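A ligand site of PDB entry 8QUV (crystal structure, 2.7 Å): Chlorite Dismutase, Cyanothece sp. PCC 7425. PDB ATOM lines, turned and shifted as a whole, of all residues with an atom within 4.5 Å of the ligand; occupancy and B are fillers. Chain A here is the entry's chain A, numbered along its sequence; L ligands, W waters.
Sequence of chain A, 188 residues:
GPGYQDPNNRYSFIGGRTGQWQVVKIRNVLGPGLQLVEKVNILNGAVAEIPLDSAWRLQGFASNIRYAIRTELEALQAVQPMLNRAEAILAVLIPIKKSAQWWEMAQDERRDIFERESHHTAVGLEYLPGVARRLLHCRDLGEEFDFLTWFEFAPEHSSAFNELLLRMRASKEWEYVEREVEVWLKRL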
ATOM      1  N   ASN A  64     -19.959 -20.953  34.682  1.00  0.00           N
ATOM      2  CA  ASN A  64     -20.122 -21.996  33.687  1.00  0.00           C
ATOM      3  C   ASN A  64     -19.365 -21.696  32.380  1.00  0.00           C
ATOM      4  O   ASN A  64     -19.078 -20.552  32.014  1.00  0.00           O
ATOM      5  CB  ASN A  64     -21.603 -22.171  33.371  1.00  0.00           C
ATOM      6  CG  ASN A  64     -22.225 -20.883  32.842  1.00  0.00           C
ATOM      7  OD1 ASN A  64     -22.474 -19.952  33.617  1.00  0.00           O
ATOM      8  ND2 ASN A  64     -22.483 -20.835  31.543  1.00  0.00           N
ATOM      9  N   ILE A  65     -19.083 -22.776  31.662  1.00  0.00           N
ATOM     10  CA  ILE A  65     -18.394 -22.748  30.391  1.00  0.00           C
ATOM     11  C   ILE A  65     -19.212 -21.902  29.414  1.00  0.00           C
ATOM     12  O   ILE A  65     -20.424 -22.002  29.408  1.00  0.00           O
ATOM     13  CB  ILE A  65     -18.199 -24.194  29.906  1.00  0.00           C
ATOM     14  CG1 ILE A  65     -17.099 -24.883  30.709  1.00  0.00           C
ATOM     15  CG2 ILE A  65     -17.938 -24.270  28.399  1.00  0.00           C
ATOM     16  CD1 ILE A  65     -15.718 -24.334  30.445  1.00  0.00           C
ATOM     17  N   ARG A  66     -18.540 -21.073  28.603  1.00  0.00           N
ATOM     18  CA  ARG A  66     -19.218 -20.214  27.633  1.00  0.00           C
ATOM     19  C   ARG A  66     -18.942 -20.604  26.165  1.00  0.00           C
ATOM     20  O   ARG A  66     -19.780 -20.255  25.328  1.00  0.00           O
ATOM     21  CB  ARG A  66     -18.824 -18.738  27.863  1.00  0.00           C
ATOM     22  CG  ARG A  66     -18.899 -18.275  29.314  1.00  0.00           C
ATOM     23  CD  ARG A  66     -20.264 -18.408  29.993  1.00  0.00           C
ATOM     24  NE  ARG A  66     -20.363 -17.801  31.320  1.00  0.00           N
ATOM     25  CZ  ARG A  66     -20.611 -16.508  31.580  1.00  0.00           C
ATOM     26  NH1 ARG A  66     -20.890 -15.668  30.582  1.00  0.00           N
ATOM     27  NH2 ARG A  66     -20.626 -16.078  32.829  1.00  0.00           N
ATOM     28  N   TYR A  67     -17.821 -21.302  25.849  1.00  0.00           N
ATOM     29  CA  TYR A  67     -17.431 -21.565  24.458  1.00  0.00           C
ATOM     30  C   TYR A  67     -17.015 -23.027  24.186  1.00  0.00           C
ATOM     31  O   TYR A  67     -17.363 -23.581  23.135  1.00  0.00           O
ATOM     32  CB  TYR A  67     -16.276 -20.659  23.994  1.00  0.00           C
ATOM     33  CG  TYR A  67     -16.680 -19.190  23.981  1.00  0.00           C
ATOM     34  CD1 TYR A  67     -17.504 -18.697  22.985  1.00  0.00           C
ATOM     35  CD2 TYR A  67     -16.306 -18.347  25.019  1.00  0.00           C
ATOM     36  CE1 TYR A  67     -17.912 -17.383  22.996  1.00  0.00           C
ATOM     37  CE2 TYR A  67     -16.714 -17.023  25.047  1.00  0.00           C
ATOM     38  CZ  TYR A  67     -17.528 -16.543  24.036  1.00  0.00           C
ATOM     39  OH  TYR A  67     -17.940 -15.222  24.078  1.00  0.00           O
ATOM     40  N   ALA A  68     -16.259 -23.622  25.113  1.00  0.00           N
ATOM     41  CA  ALA A  68     -15.726 -24.966  24.947  1.00  0.00           C
ATOM     42  C   ALA A  68     -16.817 -25.993  24.642  1.00  0.00           C
ATOM     43  O   ALA A  68     -17.836 -26.044  25.324  1.00  0.00           O
ATOM     44  CB  ALA A  68     -14.995 -25.352  26.204  1.00  0.00           C
ATOM     45  N   LEU A  76      -9.042 -31.019  27.634  1.00  0.00           N
ATOM     46  CA  LEU A  76      -8.538 -30.230  28.744  1.00  0.00           C
ATOM     47  C   LEU A  76      -8.437 -31.088  30.008  1.00  0.00           C
ATOM     48  O   LEU A  76      -7.457 -30.991  30.715  1.00  0.00           O
ATOM     49  CB  LEU A  76      -9.433 -28.998  28.948  1.00  0.00           C
ATOM     50  CG  LEU A  76      -9.410 -28.011  27.772  1.00  0.00           C
ATOM     51  CD1 LEU A  76     -10.562 -27.030  27.867  1.00  0.00           C
ATOM     52  CD2 LEU A  76      -8.084 -27.253  27.718  1.00  0.00           C
ATOM     53  N   ILE A  94      -3.671 -11.829  34.919  1.00  0.00           N
ATOM     54  CA  ILE A  94      -3.791 -10.990  33.736  1.00  0.00           C
ATOM     55  C   ILE A  94      -5.233 -10.573  33.550  1.00  0.00           C
ATOM     56  O   ILE A  94      -6.026 -11.326  32.989  1.00  0.00           O
ATOM     57  CB  ILE A  94      -3.224 -11.626  32.447  1.00  0.00           C
ATOM     58  CG1 ILE A  94      -1.828 -12.196  32.655  1.00  0.00           C
ATOM     59  CG2 ILE A  94      -3.265 -10.630  31.287  1.00  0.00           C
ATOM     60  CD1 ILE A  94      -1.335 -12.974  31.451  1.00  0.00           C
ATOM     61  N   ILE A  96      -8.172  -8.618  31.649  1.00  0.00           N
ATOM     62  CA  ILE A  96      -8.483  -8.356  30.265  1.00  0.00           C
ATOM     63  C   ILE A  96      -9.860  -7.704  30.183  1.00  0.00           C
ATOM     64  O   ILE A  96     -10.814  -8.203  30.776  1.00  0.00           O
ATOM     65  CB  ILE A  96      -8.468  -9.669  29.462  1.00  0.00           C
ATOM     66  CG1 ILE A  96      -7.038 -10.196  29.316  1.00  0.00           C
ATOM     67  CG2 ILE A  96      -9.117  -9.475  28.102  1.00  0.00           C
ATOM     68  CD1 ILE A  96      -6.996 -11.671  29.116  1.00  0.00           C
ATOM     69  N   LYS A  98     -12.432  -6.674  26.919  1.00  0.00           N
ATOM     70  CA  LYS A  98     -12.709  -6.750  25.485  1.00  0.00           C
ATOM     71  C   LYS A  98     -13.630  -5.594  25.079  1.00  0.00           C
ATOM     72  O   LYS A  98     -14.222  -4.954  25.932  1.00  0.00           O
ATOM     73  CB  LYS A  98     -13.332  -8.106  25.189  1.00  0.00           C
ATOM     74  CG  LYS A  98     -12.371  -9.278  25.289  1.00  0.00           C
ATOM     75  CD  LYS A  98     -12.845 -10.504  24.529  1.00  0.00           C
ATOM     76  CE  LYS A  98     -11.953 -11.711  24.731  1.00  0.00           C
ATOM     77  NZ  LYS A  98     -12.545 -12.978  24.218  1.00  0.00           N
ATOM     78  N   TRP A 102     -16.993  -6.494  20.485  1.00  0.00           N
ATOM     79  CA  TRP A 102     -16.981  -7.903  20.842  1.00  0.00           C
ATOM     80  C   TRP A 102     -18.290  -8.246  21.533  1.00  0.00           C
ATOM     81  O   TRP A 102     -18.967  -9.197  21.142  1.00  0.00           O
ATOM     82  CB  TRP A 102     -15.796  -8.247  21.740  1.00  0.00           C
ATOM     83  CG  TRP A 102     -15.842  -9.654  22.307  1.00  0.00           C
ATOM     84  CD1 TRP A 102     -16.262 -10.028  23.559  1.00  0.00           C
ATOM     85  CD2 TRP A 102     -15.406 -10.861  21.657  1.00  0.00           C
ATOM     86  NE1 TRP A 102     -16.155 -11.379  23.706  1.00  0.00           N
ATOM     87  CE2 TRP A 102     -15.622 -11.922  22.570  1.00  0.00           C
ATOM     88  CE3 TRP A 102     -14.861 -11.159  20.406  1.00  0.00           C
ATOM     89  CZ2 TRP A 102     -15.301 -13.243  22.270  1.00  0.00           C
ATOM     90  CZ3 TRP A 102     -14.534 -12.459  20.104  1.00  0.00           C
ATOM     91  CH2 TRP A 102     -14.763 -13.487  21.022  1.00  0.00           C
ATOM     92  N   PHE A 114     -13.108 -17.048  18.514  1.00  0.00           N
ATOM     93  CA  PHE A 114     -12.388 -17.597  19.659  1.00  0.00           C
ATOM     94  C   PHE A 114     -11.631 -18.872  19.279  1.00  0.00           C
ATOM     95  O   PHE A 114     -10.470 -19.032  19.654  1.00  0.00           O
ATOM     96  CB  PHE A 114     -13.379 -17.818  20.808  1.00  0.00           C
ATOM     97  CG  PHE A 114     -12.807 -18.517  22.018  1.00  0.00           C
ATOM     98  CD1 PHE A 114     -12.117 -17.798  22.986  1.00  0.00           C
ATOM     99  CD2 PHE A 114     -12.937 -19.880  22.181  1.00  0.00           C
ATOM    100  CE1 PHE A 114     -11.560 -18.434  24.087  1.00  0.00           C
ATOM    101  CE2 PHE A 114     -12.367 -20.515  23.270  1.00  0.00           C
ATOM    102  CZ  PHE A 114     -11.684 -19.791  24.222  1.00  0.00           C
ATOM    103  N   HIS A 120      -7.872 -20.692  20.268  1.00  0.00           N
ATOM    104  CA  HIS A 120      -7.532 -20.403  21.667  1.00  0.00           C
ATOM    105  C   HIS A 120      -7.237 -21.688  22.446  1.00  0.00           C
ATOM    106  O   HIS A 120      -6.228 -21.772  23.136  1.00  0.00           O
ATOM    107  CB  HIS A 120      -8.613 -19.555  22.338  1.00  0.00           C
ATOM    108  CG  HIS A 120      -8.293 -19.071  23.723  1.00  0.00           C
ATOM    109  ND1 HIS A 120      -8.162 -17.745  24.029  1.00  0.00           N
ATOM    110  CD2 HIS A 120      -8.106 -19.738  24.908  1.00  0.00           C
ATOM    111  CE1 HIS A 120      -7.888 -17.616  25.326  1.00  0.00           C
ATOM    112  NE2 HIS A 120      -7.825 -18.818  25.874  1.00  0.00           N
ATOM    113  N   THR A 121      -8.105 -22.695  22.331  1.00  0.00           N
ATOM    114  CA  THR A 121      -7.996 -23.898  23.150  1.00  0.00           C
ATOM    115  C   THR A 121      -6.892 -24.810  22.612  1.00  0.00           C
ATOM    116  O   THR A 121      -6.116 -25.359  23.383  1.00  0.00           O
ATOM    117  CB  THR A 121      -9.341 -24.615  23.260  1.00  0.00           C
ATOM    118  OG1 THR A 121     -10.374 -23.705  23.636  1.00  0.00           O
ATOM    119  CG2 THR A 121      -9.298 -25.732  24.283  1.00  0.00           C
ATOM    120  N   GLY A 124      -3.584 -23.120  23.606  1.00  0.00           N
ATOM    121  CA  GLY A 124      -3.406 -23.211  25.047  1.00  0.00           C
ATOM    122  C   GLY A 124      -3.037 -24.613  25.535  1.00  0.00           C
ATOM    123  O   GLY A 124      -2.232 -24.747  26.463  1.00  0.00           O
ATOM    124  N   LEU A 125      -3.614 -25.637  24.885  1.00  0.00           N
ATOM    125  CA  LEU A 125      -3.361 -27.046  25.188  1.00  0.00           C
ATOM    126  C   LEU A 125      -1.901 -27.432  24.968  1.00  0.00           C
ATOM    127  O   LEU A 125      -1.415 -28.396  25.565  1.00  0.00           O
ATOM    128  CB  LEU A 125      -4.280 -27.917  24.333  1.00  0.00           C
ATOM    129  CG  LEU A 125      -5.470 -28.542  25.058  1.00  0.00           C
ATOM    130  CD1 LEU A 125      -6.300 -29.356  24.088  1.00  0.00           C
ATOM    131  CD2 LEU A 125      -5.011 -29.431  26.206  1.00  0.00           C
ATOM    132  N   LEU A 128       0.022 -27.171  28.381  1.00  0.00           N
ATOM    133  CA  LEU A 128      -0.382 -28.014  29.498  1.00  0.00           C
ATOM    134  C   LEU A 128       0.418 -29.314  29.427  1.00  0.00           C
ATOM    135  O   LEU A 128       0.742 -29.714  28.318  1.00  0.00           O
ATOM    136  CB  LEU A 128      -1.883 -28.283  29.379  1.00  0.00           C
ATOM    137  CG  LEU A 128      -2.770 -27.354  30.203  1.00  0.00           C
ATOM    138  CD1 LEU A 128      -2.376 -25.906  30.040  1.00  0.00           C
ATOM    139  CD2 LEU A 128      -4.226 -27.549  29.828  1.00  0.00           C
ATOM    140  N   VAL A 131       1.475 -25.395  32.689  1.00  0.00           N
ATOM    141  CA  VAL A 131       0.684 -24.259  33.164  1.00  0.00           C
ATOM    142  C   VAL A 131      -0.683 -24.652  33.756  1.00  0.00           C
ATOM    143  O   VAL A 131      -1.565 -25.161  33.056  1.00  0.00           O
ATOM    144  CB  VAL A 131       0.446 -23.224  32.048  1.00  0.00           C
ATOM    145  CG1 VAL A 131      -0.352 -22.045  32.568  1.00  0.00           C
ATOM    146  CG2 VAL A 131       1.753 -22.780  31.401  1.00  0.00           C
ATOM    147  N   ARG A 133      -4.260 -22.877  35.423  1.00  0.00           N
ATOM    148  CA  ARG A 133      -5.025 -21.661  35.113  1.00  0.00           C
ATOM    149  C   ARG A 133      -6.334 -21.621  35.909  1.00  0.00           C
ATOM    150  O   ARG A 133      -6.867 -22.643  36.302  1.00  0.00           O
ATOM    151  CB  ARG A 133      -5.295 -21.562  33.606  1.00  0.00           C
ATOM    152  CG  ARG A 133      -6.347 -22.521  33.072  1.00  0.00           C
ATOM    153  CD  ARG A 133      -6.408 -22.629  31.555  1.00  0.00           C
ATOM    154  NE  ARG A 133      -7.640 -23.285  31.126  1.00  0.00           N
ATOM    155  CZ  ARG A 133      -7.887 -24.593  31.206  1.00  0.00           C
ATOM    156  NH1 ARG A 133      -6.939 -25.438  31.574  1.00  0.00           N
ATOM    157  NH2 ARG A 133      -9.076 -25.071  30.915  1.00  0.00           N
ATOM    158  N   LEU A 135     -10.069 -19.107  35.575  1.00  0.00           N
ATOM    159  CA  LEU A 135     -10.711 -18.034  34.839  1.00  0.00           C
ATOM    160  C   LEU A 135     -11.893 -17.476  35.638  1.00  0.00           C
ATOM    161  O   LEU A 135     -12.798 -18.212  36.072  1.00  0.00           O
ATOM    162  CB  LEU A 135     -11.161 -18.523  33.466  1.00  0.00           C
ATOM    163  CG  LEU A 135     -12.030 -17.545  32.677  1.00  0.00           C
ATOM    164  CD1 LEU A 135     -11.274 -16.278  32.338  1.00  0.00           C
ATOM    165  CD2 LEU A 135     -12.567 -18.176  31.401  1.00  0.00           C
ATOM    166  N   PHE A 147     -12.394  -9.591  32.594  1.00  0.00           N
ATOM    167  CA  PHE A 147     -11.919 -10.900  33.038  1.00  0.00           C
ATOM    168  C   PHE A 147     -10.652 -10.782  33.878  1.00  0.00           C
ATOM    169  O   PHE A 147      -9.837  -9.920  33.659  1.00  0.00           O
ATOM    170  CB  PHE A 147     -11.551 -11.836  31.881  1.00  0.00           C
ATOM    171  CG  PHE A 147     -12.612 -12.033  30.835  1.00  0.00           C
ATOM    172  CD1 PHE A 147     -13.701 -12.856  31.050  1.00  0.00           C
ATOM    173  CD2 PHE A 147     -12.504 -11.384  29.620  1.00  0.00           C
ATOM    174  CE1 PHE A 147     -14.672 -13.024  30.069  1.00  0.00           C
ATOM    175  CE2 PHE A 147     -13.475 -11.551  28.639  1.00  0.00           C
ATOM    176  CZ  PHE A 147     -14.561 -12.351  28.875  1.00  0.00           C
ATOM    177  N   THR A 149      -7.624 -13.472  34.660  1.00  0.00           N
ATOM    178  CA  THR A 149      -7.062 -14.756  34.305  1.00  0.00           C
ATOM    179  C   THR A 149      -5.878 -14.978  35.222  1.00  0.00           C
ATOM    180  O   THR A 149      -5.239 -14.032  35.640  1.00  0.00           O
ATOM    181  CB  THR A 149      -6.728 -14.829  32.808  1.00  0.00           C
ATOM    182  OG1 THR A 149      -5.639 -13.977  32.459  1.00  0.00           O
ATOM    183  CG2 THR A 149      -7.926 -14.502  31.955  1.00  0.00           C
ATOM    184  N   PHE A 151      -2.614 -17.800  36.135  1.00  0.00           N
ATOM    185  CA  PHE A 151      -1.758 -18.841  35.614  1.00  0.00           C
ATOM    186  C   PHE A 151      -0.632 -19.080  36.588  1.00  0.00           C
ATOM    187  O   PHE A 151      -0.047 -18.107  37.059  1.00  0.00           O
ATOM    188  CB  PHE A 151      -1.127 -18.433  34.286  1.00  0.00           C
ATOM    189  CG  PHE A 151      -2.164 -18.024  33.303  1.00  0.00           C
ATOM    190  CD1 PHE A 151      -2.855 -18.973  32.582  1.00  0.00           C
ATOM    191  CD2 PHE A 151      -2.524 -16.689  33.196  1.00  0.00           C
ATOM    192  CE1 PHE A 151      -3.848 -18.581  31.681  1.00  0.00           C
ATOM    193  CE2 PHE A 151      -3.553 -16.311  32.350  1.00  0.00           C
ATOM    194  CZ  PHE A 151      -4.190 -17.251  31.577  1.00  0.00           C
ATOM    195  N   PHE A 161       5.641 -19.963  28.914  1.00  0.00           N
ATOM    196  CA  PHE A 161       4.499 -19.115  29.220  1.00  0.00           C
ATOM    197  C   PHE A 161       4.590 -17.808  28.435  1.00  0.00           C
ATOM    198  O   PHE A 161       3.580 -17.336  27.918  1.00  0.00           O
ATOM    199  CB  PHE A 161       4.339 -18.858  30.724  1.00  0.00           C
ATOM    200  CG  PHE A 161       3.084 -18.077  31.034  1.00  0.00           C
ATOM    201  CD1 PHE A 161       1.845 -18.665  30.916  1.00  0.00           C
ATOM    202  CD2 PHE A 161       3.157 -16.713  31.304  1.00  0.00           C
ATOM    203  CE1 PHE A 161       0.683 -17.931  31.104  1.00  0.00           C
ATOM    204  CE2 PHE A 161       2.001 -15.985  31.508  1.00  0.00           C
ATOM    205  CZ  PHE A 161       0.769 -16.589  31.387  1.00  0.00           C
ATOM    206  N   LEU A 164       3.593 -18.413  24.967  1.00  0.00           N
ATOM    207  CA  LEU A 164       2.130 -18.477  24.887  1.00  0.00           C
ATOM    208  C   LEU A 164       1.506 -17.075  24.828  1.00  0.00           C
ATOM    209  O   LEU A 164       0.641 -16.825  23.993  1.00  0.00           O
ATOM    210  CB  LEU A 164       1.599 -19.332  26.045  1.00  0.00           C
ATOM    211  CG  LEU A 164       0.103 -19.266  26.342  1.00  0.00           C
ATOM    212  CD1 LEU A 164      -0.727 -19.899  25.226  1.00  0.00           C
ATOM    213  CD2 LEU A 164      -0.215 -19.904  27.688  1.00  0.00           C
ATOM    214  N   LEU A 165       1.958 -16.117  25.658  1.00  0.00           N
ATOM    215  CA  LEU A 165       1.363 -14.789  25.679  1.00  0.00           C
ATOM    216  C   LEU A 165       1.466 -14.143  24.314  1.00  0.00           C
ATOM    217  O   LEU A 165       0.532 -13.492  23.877  1.00  0.00           O
ATOM    218  CB  LEU A 165       2.085 -13.891  26.679  1.00  0.00           C
ATOM    219  CG  LEU A 165       1.794 -14.138  28.161  1.00  0.00           C
ATOM    220  CD1 LEU A 165       2.726 -13.266  29.003  1.00  0.00           C
ATOM    221  CD2 LEU A 165       0.344 -13.842  28.541  1.00  0.00           C
ATOM    222  N   MET A 168      -1.008 -15.652  21.701  1.00  0.00           N
ATOM    223  CA  MET A 168      -2.395 -15.278  21.906  1.00  0.00           C
ATOM    224  C   MET A 168      -2.614 -13.859  21.375  1.00  0.00           C
ATOM    225  O   MET A 168      -3.623 -13.596  20.717  1.00  0.00           O
ATOM    226  CB  MET A 168      -2.771 -15.334  23.387  1.00  0.00           C
ATOM    227  CG  MET A 168      -2.859 -16.751  23.993  1.00  0.00           C
ATOM    228  SD  MET A 168      -4.317 -17.663  23.447  1.00  0.00           S
ATOM    229  CE  MET A 168      -4.411 -18.945  24.698  1.00  0.00           C
ATOM    230  N   GLU A 173      -8.685 -12.963  17.970  1.00  0.00           N
ATOM    231  CA  GLU A 173      -9.362 -12.684  19.229  1.00  0.00           C
ATOM    232  C   GLU A 173      -8.825 -11.396  19.846  1.00  0.00           C
ATOM    233  O   GLU A 173      -9.595 -10.588  20.359  1.00  0.00           O
ATOM    234  CB  GLU A 173      -9.178 -13.856  20.206  1.00  0.00           C
ATOM    235  CG  GLU A 173     -10.033 -13.770  21.463  1.00  0.00           C
ATOM    236  CD  GLU A 173      -9.718 -14.844  22.500  1.00  0.00           C
ATOM    237  OE1 GLU A 173      -8.808 -15.656  22.250  1.00  0.00           O
ATOM    238  OE2 GLU A 173     -10.393 -14.870  23.582  1.00  0.00           O
ATOM    239  N   TRP A 174      -7.497 -11.199  19.819  1.00  0.00           N
ATOM    240  CA  TRP A 174      -6.878 -10.150  20.618  1.00  0.00           C
ATOM    241  C   TRP A 174      -7.026  -8.767  19.993  1.00  0.00           C
ATOM    242  O   TRP A 174      -6.661  -7.797  20.626  1.00  0.00           O
ATOM    243  CB  TRP A 174      -5.411 -10.454  20.946  1.00  0.00           C
ATOM    244  CG  TRP A 174      -5.177 -10.628  22.428  1.00  0.00           C
ATOM    245  CD1 TRP A 174      -4.598  -9.706  23.257  1.00  0.00           C
ATOM    246  CD2 TRP A 174      -5.464 -11.776  23.253  1.00  0.00           C
ATOM    247  NE1 TRP A 174      -4.519 -10.208  24.526  1.00  0.00           N
ATOM    248  CE2 TRP A 174      -5.039 -11.471  24.551  1.00  0.00           C
ATOM    249  CE3 TRP A 174      -6.042 -13.039  23.019  1.00  0.00           C
ATOM    250  CZ2 TRP A 174      -5.186 -12.364  25.621  1.00  0.00           C
ATOM    251  CZ3 TRP A 174      -6.174 -13.929  24.064  1.00  0.00           C
ATOM    252  CH2 TRP A 174      -5.758 -13.589  25.352  1.00  0.00           C
ATOM    253  N   GLU A 180      -5.196  -4.525  29.001  1.00  0.00           N
ATOM    254  CA  GLU A 180      -4.493  -5.704  29.475  1.00  0.00           C
ATOM    255  C   GLU A 180      -3.326  -5.290  30.379  1.00  0.00           C
ATOM    256  O   GLU A 180      -2.684  -4.270  30.130  1.00  0.00           O
ATOM    257  CB  GLU A 180      -4.003  -6.523  28.284  1.00  0.00           C
ATOM    258  CG  GLU A 180      -3.429  -7.863  28.656  1.00  0.00           C
ATOM    259  CD  GLU A 180      -3.096  -8.759  27.463  1.00  0.00           C
ATOM    260  OE1 GLU A 180      -3.263  -8.297  26.275  1.00  0.00           O
ATOM    261  OE2 GLU A 180      -2.667  -9.916  27.743  1.00  0.00           O
HETATM  262  C1  LIG L   1     -11.176 -18.618  27.980  1.00  0.00           C
HETATM  263  C2  LIG L   1      -8.223 -22.368  27.673  1.00  0.00           C
HETATM  264  C3  LIG L   1      -4.404 -19.511  28.314  1.00  0.00           C
HETATM  265  C4  LIG L   1      -7.358 -15.699  28.196  1.00  0.00           C
HETATM  266  C5  LIG L   1     -10.666 -19.890  27.817  1.00  0.00           C
HETATM  267  C6  LIG L   1     -11.468 -21.000  27.473  1.00  0.00           C
HETATM  268  C7  LIG L   1     -10.624 -22.062  27.398  1.00  0.00           C
HETATM  269  C8  LIG L   1      -9.328 -21.582  27.678  1.00  0.00           C
HETATM  270  C9  LIG L   1     -10.974 -23.488  27.056  1.00  0.00           C
HETATM  271  C10 LIG L   1     -12.952 -21.048  27.243  1.00  0.00           C
HETATM  272  C11 LIG L   1     -13.722 -21.084  28.552  1.00  0.00           C
HETATM  273  C12 LIG L   1     -15.237 -21.214  28.371  1.00  0.00           C
HETATM  274  O1  LIG L   1     -15.916 -20.705  29.279  1.00  0.00           O
HETATM  275  O2  LIG L   1     -15.812 -21.816  27.405  1.00  0.00           O
HETATM  276  C13 LIG L   1      -6.958 -21.903  27.867  1.00  0.00           C
HETATM  277  C14 LIG L   1      -5.881 -22.801  27.965  1.00  0.00           C
HETATM  278  C15 LIG L   1      -4.785 -22.034  28.148  1.00  0.00           C
HETATM  279  C16 LIG L   1      -5.232 -20.625  28.171  1.00  0.00           C
HETATM  280  C17 LIG L   1      -5.874 -24.307  27.913  1.00  0.00           C
HETATM  281  C18 LIG L   1      -3.476 -22.628  28.405  1.00  0.00           C
HETATM  282  C19 LIG L   1      -2.582 -21.950  29.108  1.00  0.00           C
HETATM  283  C20 LIG L   1      -4.860 -18.196  28.299  1.00  0.00           C
HETATM  284  C21 LIG L   1      -4.071 -17.024  28.452  1.00  0.00           C
HETATM  285  C22 LIG L   1      -4.930 -15.964  28.434  1.00  0.00           C
HETATM  286  C23 LIG L   1      -6.232 -16.483  28.249  1.00  0.00           C
HETATM  287  C24 LIG L   1      -2.594 -16.917  28.634  1.00  0.00           C
HETATM  288  C25 LIG L   1      -4.644 -14.544  28.544  1.00  0.00           C
HETATM  289  C26 LIG L   1      -3.433 -14.028  28.648  1.00  0.00           C
HETATM  290  C27 LIG L   1      -8.633 -16.217  28.151  1.00  0.00           C
HETATM  291  C28 LIG L   1      -9.844 -15.368  28.256  1.00  0.00           C
HETATM  292  C29 LIG L   1     -10.896 -16.195  28.204  1.00  0.00           C
HETATM  293  C30 LIG L   1     -10.329 -17.526  28.101  1.00  0.00           C
HETATM  294  C31 LIG L   1      -9.924 -13.845  28.390  1.00  0.00           C
HETATM  295  C32 LIG L   1     -12.329 -15.784  28.256  1.00  0.00           C
HETATM  296  C33 LIG L   1     -12.810 -15.378  26.863  1.00  0.00           C
HETATM  297  C34 LIG L   1     -14.269 -14.967  26.880  1.00  0.00           C
HETATM  298  O3  LIG L   1     -15.109 -15.542  27.662  1.00  0.00           O
HETATM  299  O4  LIG L   1     -14.596 -14.041  26.098  1.00  0.00           O
HETATM  300  N1  LIG L   1      -9.323 -20.252  27.931  1.00  0.00           N
HETATM  301  N2  LIG L   1      -6.546 -20.660  28.006  1.00  0.00           N
HETATM  302  N3  LIG L   1      -6.139 -17.844  28.167  1.00  0.00           N
HETATM  303  N4  LIG L   1      -8.975 -17.508  28.078  1.00  0.00           N
HETATM  304 FE1  LIG L   1      -7.788 -19.007  27.959  1.00  0.00          FE
HETATM  305  O   HOH W   1      -8.241 -19.595  30.889  1.00  0.00           O
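An iron atom (FE1) of the ligand is bound by a ring nitrogen (NE2) of His 120, 2.1 Å away.
O2 of the ligand is in hydrogen-bond range of N of Tyr 67 (2.6 Å).
The backbone NH (N) of Arg 66 lies within hydrogen-bond range of an oxygen (O1) of the ligand.
N of Ala 68 lies within hydrogen-bond range of O2 of the ligand, 3.0 Å away.
The side-chain amino group (NZ) of Lys 98 is in salt-bridge range of an oxygen (O4) of the ligand (3.0 Å).
The backbone NH of His 120 sits at hydrogen-bond distance from the backbone carbonyl oxygen of Phe 114.
The side-chain carboxylate (OE1) of Glu 173 is in hydrogen-bond range of a ring nitrogen (ND1) of His 120 (2.8 Å).
NE of Arg 66 lies within hydrogen-bond range of O of Asn 64 (3.1 Å).
The side-chain amino group (NZ) of Lys 98 lies within salt-bridge range of the side-chain carboxylate (OE2) of Glu 173, at 2.9 Å.
The backbone NH (N) of Phe 147 lies within hydrogen-bond range of the backbone carbonyl oxygen (O) of Ile 96 (2.8 Å).
NE1 of Trp 174 sits at hydrogen-bond distance from OE1 of Glu 180.
The backbone carbonyl oxygen (O) of Ile 94 sits at hydrogen-bond distance from the side-chain hydroxyl (OG1) of Thr 149 (2.7 Å).
Residues that only touch the ligand: Ile 65, Leu 76, Ile 94, Ile 96, Trp 102, Phe 114, Thr 121, Gly 124, Leu 128, Arg 133, Leu 135, Phe 147, Thr 149, Phe 151, Leu 164, Leu 165, Met 168 and Trp 174.
Within 4 Å of the ligand: Ile 65, Arg 66, Tyr 67, Ala 68, Leu 76, Ile 94, Ile 96, Lys 98, Trp 102, Phe 114, His 120, Thr 121, Gly 124, Leu 128, Arg 133, Leu 135, Phe 147, Thr 149, Phe 151, Leu 164, Leu 165, Met 168 and Trp 174.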
